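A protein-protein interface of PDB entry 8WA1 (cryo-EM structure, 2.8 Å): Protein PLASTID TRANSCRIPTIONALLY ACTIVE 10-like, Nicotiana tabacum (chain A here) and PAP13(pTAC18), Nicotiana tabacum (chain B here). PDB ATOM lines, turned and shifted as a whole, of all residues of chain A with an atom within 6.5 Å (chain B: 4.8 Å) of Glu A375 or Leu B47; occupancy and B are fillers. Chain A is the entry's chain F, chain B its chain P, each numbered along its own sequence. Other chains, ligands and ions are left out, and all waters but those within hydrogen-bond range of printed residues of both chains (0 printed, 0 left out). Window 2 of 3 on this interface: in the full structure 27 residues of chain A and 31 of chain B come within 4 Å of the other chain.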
ATOM      1  N   ASP A 370     -19.234   7.136 -13.234  1.00  0.00           N
ATOM      2  CA  ASP A 370     -20.227   7.532 -14.223  1.00  0.00           C
ATOM      3  C   ASP A 370     -21.293   8.417 -13.590  1.00  0.00           C
ATOM      4  O   ASP A 370     -21.977   8.013 -12.646  1.00  0.00           O
ATOM      5  CB  ASP A 370     -20.870   6.295 -14.849  1.00  0.00           C
ATOM      6  CG  ASP A 370     -19.860   5.399 -15.536  1.00  0.00           C
ATOM      7  OD1 ASP A 370     -19.122   4.682 -14.828  1.00  0.00           O
ATOM      8  OD2 ASP A 370     -19.802   5.413 -16.783  1.00  0.00           O
ATOM      9  N   THR A 371     -21.429   9.635 -14.115  1.00  0.00           N
ATOM     10  CA  THR A 371     -22.450  10.565 -13.655  1.00  0.00           C
ATOM     11  C   THR A 371     -23.373  11.056 -14.757  1.00  0.00           C
ATOM     12  O   THR A 371     -24.437  11.603 -14.442  1.00  0.00           O
ATOM     13  CB  THR A 371     -21.807  11.782 -12.972  1.00  0.00           C
ATOM     14  OG1 THR A 371     -20.811  12.347 -13.835  1.00  0.00           O
ATOM     15  CG2 THR A 371     -21.163  11.380 -11.655  1.00  0.00           C
ATOM     16  N   ASN A 372     -23.012  10.883 -16.026  1.00  0.00           N
ATOM     17  CA  ASN A 372     -23.860  11.255 -17.152  1.00  0.00           C
ATOM     18  C   ASN A 372     -24.280   9.985 -17.874  1.00  0.00           C
ATOM     19  O   ASN A 372     -23.434   9.267 -18.418  1.00  0.00           O
ATOM     20  CB  ASN A 372     -23.136  12.209 -18.104  1.00  0.00           C
ATOM     21  CG  ASN A 372     -24.037  12.723 -19.208  1.00  0.00           C
ATOM     22  OD1 ASN A 372     -25.261  12.607 -19.132  1.00  0.00           O
ATOM     23  ND2 ASN A 372     -23.437  13.297 -20.243  1.00  0.00           N
ATOM     24  N   LEU A 373     -25.587   9.709 -17.876  1.00  0.00           N
ATOM     25  CA  LEU A 373     -26.086   8.476 -18.476  1.00  0.00           C
ATOM     26  C   LEU A 373     -25.894   8.463 -19.985  1.00  0.00           C
ATOM     27  O   LEU A 373     -25.736   7.390 -20.580  1.00  0.00           O
ATOM     28  CB  LEU A 373     -27.562   8.292 -18.127  1.00  0.00           C
ATOM     29  CG  LEU A 373     -27.911   8.442 -16.645  1.00  0.00           C
ATOM     30  CD1 LEU A 373     -29.418   8.480 -16.447  1.00  0.00           C
ATOM     31  CD2 LEU A 373     -27.287   7.320 -15.831  1.00  0.00           C
ATOM     32  N   ASP A 374     -25.907   9.636 -20.624  1.00  0.00           N
ATOM     33  CA  ASP A 374     -25.745   9.687 -22.072  1.00  0.00           C
ATOM     34  C   ASP A 374     -24.331   9.294 -22.483  1.00  0.00           C
ATOM     35  O   ASP A 374     -24.138   8.589 -23.483  1.00  0.00           O
ATOM     36  CB  ASP A 374     -26.091  11.085 -22.586  1.00  0.00           C
ATOM     37  CG  ASP A 374     -26.467  11.089 -24.054  1.00  0.00           C
ATOM     38  OD1 ASP A 374     -26.453  10.005 -24.675  1.00  0.00           O
ATOM     39  OD2 ASP A 374     -26.779  12.175 -24.586  1.00  0.00           O
ATOM     40  N   GLU A 375     -23.328   9.737 -21.721  1.00  0.00           N
ATOM     41  CA  GLU A 375     -21.957   9.315 -21.990  1.00  0.00           C
ATOM     42  C   GLU A 375     -21.803   7.811 -21.821  1.00  0.00           C
ATOM     43  O   GLU A 375     -21.113   7.157 -22.611  1.00  0.00           O
ATOM     44  CB  GLU A 375     -20.985  10.055 -21.072  1.00  0.00           C
ATOM     45  CG  GLU A 375     -20.845  11.536 -21.363  1.00  0.00           C
ATOM     46  CD  GLU A 375     -19.830  12.208 -20.461  1.00  0.00           C
ATOM     47  OE1 GLU A 375     -19.491  11.626 -19.410  1.00  0.00           O
ATOM     48  OE2 GLU A 375     -19.367  13.315 -20.807  1.00  0.00           O
ATOM     49  N   LEU A 376     -22.449   7.243 -20.799  1.00  0.00           N
ATOM     50  CA  LEU A 376     -22.403   5.799 -20.602  1.00  0.00           C
ATOM     51  C   LEU A 376     -23.055   5.067 -21.769  1.00  0.00           C
ATOM     52  O   LEU A 376     -22.527   4.061 -22.258  1.00  0.00           O
ATOM     53  CB  LEU A 376     -23.086   5.433 -19.283  1.00  0.00           C
ATOM     54  CG  LEU A 376     -23.233   3.941 -18.979  1.00  0.00           C
ATOM     55  CD1 LEU A 376     -21.874   3.262 -18.951  1.00  0.00           C
ATOM     56  CD2 LEU A 376     -23.971   3.732 -17.665  1.00  0.00           C
ATOM     57  N   ARG A 377     -24.209   5.560 -22.227  1.00  0.00           N
ATOM     58  CA  ARG A 377     -24.894   4.924 -23.348  1.00  0.00           C
ATOM     59  C   ARG A 377     -24.061   5.000 -24.620  1.00  0.00           C
ATOM     60  O   ARG A 377     -24.041   4.053 -25.416  1.00  0.00           O
ATOM     61  CB  ARG A 377     -26.260   5.573 -23.564  1.00  0.00           C
ATOM     62  N   ARG A 378     -23.369   6.121 -24.833  1.00  0.00           N
ATOM     63  CA  ARG A 378     -22.503   6.240 -26.002  1.00  0.00           C
ATOM     64  C   ARG A 378     -21.286   5.330 -25.883  1.00  0.00           C
ATOM     65  O   ARG A 378     -20.811   4.782 -26.885  1.00  0.00           O
ATOM     66  CB  ARG A 378     -22.073   7.695 -26.194  1.00  0.00           C
ATOM     67  CG  ARG A 378     -23.089   8.554 -26.931  1.00  0.00           C
ATOM     68  CD  ARG A 378     -22.550   9.955 -27.176  1.00  0.00           C
ATOM     69  NE  ARG A 378     -23.304  10.664 -28.208  1.00  0.00           N
ATOM     70  CZ  ARG A 378     -24.373  11.417 -27.969  1.00  0.00           C
ATOM     71  NH1 ARG A 378     -24.822  11.564 -26.731  1.00  0.00           N
ATOM     72  NH2 ARG A 378     -24.993  12.025 -28.971  1.00  0.00           N
ATOM     73  N   ASP A 379     -20.766   5.158 -24.665  1.00  0.00           N
ATOM     74  CA  ASP A 379     -19.582   4.327 -24.479  1.00  0.00           C
ATOM     75  C   ASP A 379     -19.905   2.848 -24.649  1.00  0.00           C
ATOM     76  O   ASP A 379     -19.119   2.099 -25.242  1.00  0.00           O
ATOM     77  CB  ASP A 379     -18.972   4.589 -23.102  1.00  0.00           C
ATOM     78  CG  ASP A 379     -17.591   3.984 -22.951  1.00  0.00           C
ATOM     79  OD1 ASP A 379     -16.977   3.633 -23.981  1.00  0.00           O
ATOM     80  OD2 ASP A 379     -17.118   3.858 -21.802  1.00  0.00           O
ATOM     81  N   CYS A 380     -21.052   2.405 -24.136  1.00  0.00           N
ATOM     82  CA  CYS A 380     -21.445   1.003 -24.207  1.00  0.00           C
ATOM     83  C   CYS A 380     -22.208   0.671 -25.483  1.00  0.00           C
ATOM     84  O   CYS A 380     -22.565  -0.493 -25.693  1.00  0.00           O
ATOM     85  CB  CYS A 380     -22.281   0.626 -22.983  1.00  0.00           C
ATOM     86  SG  CYS A 380     -23.920   1.377 -22.924  1.00  0.00           S
ATOM     87  N   LYS B  42     -10.987   7.654 -22.602  1.00  0.00           N
ATOM     88  CA  LYS B  42     -11.179   8.057 -23.988  1.00  0.00           C
ATOM     89  C   LYS B  42     -11.628   9.515 -24.038  1.00  0.00           C
ATOM     90  O   LYS B  42     -12.487   9.919 -23.246  1.00  0.00           O
ATOM     91  CB  LYS B  42     -12.208   7.150 -24.663  1.00  0.00           C
ATOM     92  CG  LYS B  42     -12.194   7.192 -26.183  1.00  0.00           C
ATOM     93  CD  LYS B  42     -12.884   5.970 -26.773  1.00  0.00           C
ATOM     94  CE  LYS B  42     -14.371   5.959 -26.465  1.00  0.00           C
ATOM     95  NZ  LYS B  42     -15.099   7.017 -27.218  1.00  0.00           N
ATOM     96  N   PRO B  43     -11.071  10.332 -24.934  1.00  0.00           N
ATOM     97  CA  PRO B  43     -11.459  11.746 -24.979  1.00  0.00           C
ATOM     98  C   PRO B  43     -12.918  11.918 -25.374  1.00  0.00           C
ATOM     99  O   PRO B  43     -13.475  11.133 -26.142  1.00  0.00           O
ATOM    100  CB  PRO B  43     -10.519  12.339 -26.036  1.00  0.00           C
ATOM    101  CG  PRO B  43     -10.124  11.173 -26.884  1.00  0.00           C
ATOM    102  CD  PRO B  43     -10.048  10.007 -25.943  1.00  0.00           C
ATOM    103  N   LEU B  44     -13.535  12.974 -24.832  1.00  0.00           N
ATOM    104  CA  LEU B  44     -14.952  13.219 -25.081  1.00  0.00           C
ATOM    105  C   LEU B  44     -15.237  13.470 -26.554  1.00  0.00           C
ATOM    106  O   LEU B  44     -16.354  13.215 -27.020  1.00  0.00           O
ATOM    107  CB  LEU B  44     -15.441  14.401 -24.246  1.00  0.00           C
ATOM    108  CG  LEU B  44     -15.605  14.189 -22.742  1.00  0.00           C
ATOM    109  CD1 LEU B  44     -16.246  15.420 -22.130  1.00  0.00           C
ATOM    110  CD2 LEU B  44     -16.432  12.947 -22.452  1.00  0.00           C
ATOM    111  N   GLU B  45     -14.253  13.983 -27.297  1.00  0.00           N
ATOM    112  CA  GLU B  45     -14.438  14.171 -28.733  1.00  0.00           C
ATOM    113  C   GLU B  45     -14.719  12.845 -29.428  1.00  0.00           C
ATOM    114  O   GLU B  45     -15.478  12.794 -30.403  1.00  0.00           O
ATOM    115  CB  GLU B  45     -13.207  14.847 -29.341  1.00  0.00           C
ATOM    116  CG  GLU B  45     -11.973  14.845 -28.450  1.00  0.00           C
ATOM    117  CD  GLU B  45     -11.950  16.014 -27.481  1.00  0.00           C
ATOM    118  OE1 GLU B  45     -12.863  16.863 -27.547  1.00  0.00           O
ATOM    119  OE2 GLU B  45     -11.017  16.084 -26.653  1.00  0.00           O
ATOM    120  N   GLU B  46     -14.119  11.759 -28.937  1.00  0.00           N
ATOM    121  CA  GLU B  46     -14.370  10.448 -29.526  1.00  0.00           C
ATOM    122  C   GLU B  46     -15.755   9.930 -29.156  1.00  0.00           C
ATOM    123  O   GLU B  46     -16.430   9.302 -29.981  1.00  0.00           O
ATOM    124  CB  GLU B  46     -13.290   9.461 -29.083  1.00  0.00           C
ATOM    125  CG  GLU B  46     -13.321   8.135 -29.823  1.00  0.00           C
ATOM    126  CD  GLU B  46     -12.962   8.277 -31.291  1.00  0.00           C
ATOM    127  OE1 GLU B  46     -12.292   9.268 -31.651  1.00  0.00           O
ATOM    128  OE2 GLU B  46     -13.348   7.395 -32.087  1.00  0.00           O
ATOM    129  N   LEU B  47     -16.196  10.180 -27.918  1.00  0.00           N
ATOM    130  CA  LEU B  47     -17.502   9.689 -27.485  1.00  0.00           C
ATOM    131  C   LEU B  47     -18.633  10.349 -28.264  1.00  0.00           C
ATOM    132  O   LEU B  47     -19.538   9.667 -28.758  1.00  0.00           O
ATOM    133  CB  LEU B  47     -17.688   9.923 -25.985  1.00  0.00           C
ATOM    134  CG  LEU B  47     -17.072   8.923 -25.002  1.00  0.00           C
ATOM    135  CD1 LEU B  47     -15.586   9.172 -24.807  1.00  0.00           C
ATOM    136  CD2 LEU B  47     -17.803   8.966 -23.669  1.00  0.00           C
ATOM    137  N   TYR B  48     -18.596  11.674 -28.392  1.00  0.00           N
ATOM    138  CA  TYR B  48     -19.643  12.423 -29.071  1.00  0.00           C
ATOM    139  C   TYR B  48     -19.352  12.627 -30.551  1.00  0.00           C
ATOM    140  O   TYR B  48     -20.033  13.428 -31.200  1.00  0.00           O
ATOM    141  CB  TYR B  48     -19.858  13.772 -28.383  1.00  0.00           C
ATOM    142  CG  TYR B  48     -20.580  13.673 -27.057  1.00  0.00           C
ATOM    143  CD1 TYR B  48     -19.890  13.379 -25.889  1.00  0.00           C
ATOM    144  CD2 TYR B  48     -21.953  13.868 -26.977  1.00  0.00           C
ATOM    145  CE1 TYR B  48     -20.547  13.285 -24.678  1.00  0.00           C
ATOM    146  CE2 TYR B  48     -22.617  13.777 -25.769  1.00  0.00           C
ATOM    147  CZ  TYR B  48     -21.910  13.483 -24.624  1.00  0.00           C
ATOM    148  OH  TYR B  48     -22.568  13.393 -23.420  1.00  0.00           O
ATOM    149  N   ASN B  49     -18.355  11.921 -31.091  1.00  0.00           N
ATOM    150  CA  ASN B  49     -18.020  11.966 -32.516  1.00  0.00           C
ATOM    151  C   ASN B  49     -17.701  13.390 -32.967  1.00  0.00           C
ATOM    152  O   ASN B  49     -18.014  13.793 -34.089  1.00  0.00           O
ATOM    153  CB  ASN B  49     -19.139  11.357 -33.365  1.00  0.00           C
ATOM    154  CG  ASN B  49     -18.668  10.949 -34.748  1.00  0.00           C
ATOM    155  OD1 ASN B  49     -18.899  11.653 -35.729  1.00  0.00           O
ATOM    156  ND2 ASN B  49     -18.001   9.803 -34.831  1.00  0.00           N
ATOM    157  N   PRO B 100     -20.854  18.733 -22.716  1.00  0.00           N
ATOM    158  CA  PRO B 100     -22.061  18.038 -23.171  1.00  0.00           C
ATOM    159  C   PRO B 100     -23.203  18.219 -22.185  1.00  0.00           C
ATOM    160  O   PRO B 100     -22.999  18.554 -21.015  1.00  0.00           O
ATOM    161  CB  PRO B 100     -21.624  16.571 -23.249  1.00  0.00           C
ATOM    162  CG  PRO B 100     -20.128  16.610 -23.296  1.00  0.00           C
ATOM    163  CD  PRO B 100     -19.737  17.804 -22.483  1.00  0.00           C
ATOM    164  N   SER B 103     -23.136  16.581 -18.620  1.00  0.00           N
ATOM    165  CA  SER B 103     -21.791  16.081 -18.376  1.00  0.00           C
ATOM    166  C   SER B 103     -21.002  17.066 -17.524  1.00  0.00           C
ATOM    167  O   SER B 103     -21.128  18.283 -17.684  1.00  0.00           O
ATOM    168  CB  SER B 103     -21.058  15.829 -19.694  1.00  0.00           C
ATOM    169  OG  SER B 103     -19.745  15.346 -19.465  1.00  0.00           O
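Among the printed residues, merely in contact across the chains: Asn A372 with Ser B103 (3.5 Å), Glu A375 with Leu B44 (3.4 Å), Glu A375 with Leu B47 (3.9 Å), Glu A375 with Tyr B48 (3.3 Å), Arg A378 with Leu B47 (3.4 Å) and Arg A378 with Tyr B48 (3.3 Å).
Printed residues of chain A that touch a printed residue of chain B: Asn A372, Glu A375 and Arg A378.
Of the 10 printed residues of chain B, 4 touch a printed residue of chain A.
Printed residues of chain B that touch a printed residue of chain A: Leu B44, Leu B47, Tyr B48 and Ser B103.
Hydrophobic or aromatic side chains of chain B that line the printed part of chain A: Leu B44, Leu B47 and Tyr B48.
Along chain B the printed residues that touch a printed residue of chain A span positions 44 to 103.
Among the printed residues, 8 pairs touch across the chains.
Among the printed residues, no Asp or Glu carboxylate lies within 4 Å of a Lys or Arg side-chain nitrogen of the other chain.
Of chain B, only Leu B44 (3.4 Å), Leu B47 (3.9 Å), Tyr B48 (3.3 Å) and Ser B103 (2.5 Å) come within 4 Å of Glu A375.
Printed residues of chain B within 4 Å of Arg A378: Leu B47 (3.4 Å) and Tyr B48 (3.3 Å).
Cys A380 touches none of the printed residues of chain B.
Of the printed residues of chain A, Leu B44 touches Glu A375 (3.4 Å).
Of chain A, only Glu A375 (3.9 Å) and Arg A378 (3.4 Å) come within 4 Å of Leu B47.
Printed residues of chain A within 4 Å of Tyr B48: Asn A372, Glu A375 and Arg A378.
Of the printed residues of chain A, Ser B103 touches Asn A372 (3.5 Å) and Glu A375 (2.5 Å).
The nearest residue of chain B that does not touch Glu A375 is Pro B100 (4.2 Å).
The nearest residue of chain A that does not touch Leu B47 is Asp A379 (4.6 Å).
The side-chain hydroxyl (OH) of Tyr B48 sits at hydrogen-bond distance from the side-chain amide nitrogen (ND2) of Asn A372 (3.3 Å).
The side-chain hydroxyl (OG) of Ser B103 sits at hydrogen-bond distance from the side-chain carboxylate (OE2) of Glu A375 (2.5 Å).
NH1 of Arg A378 is in salt-bridge range of OD2 of Asp A374 (3.0 Å).
The side-chain amide oxygen of Asn A372 sits close to the backbone NH of Asp A374, 3.4 Å away.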
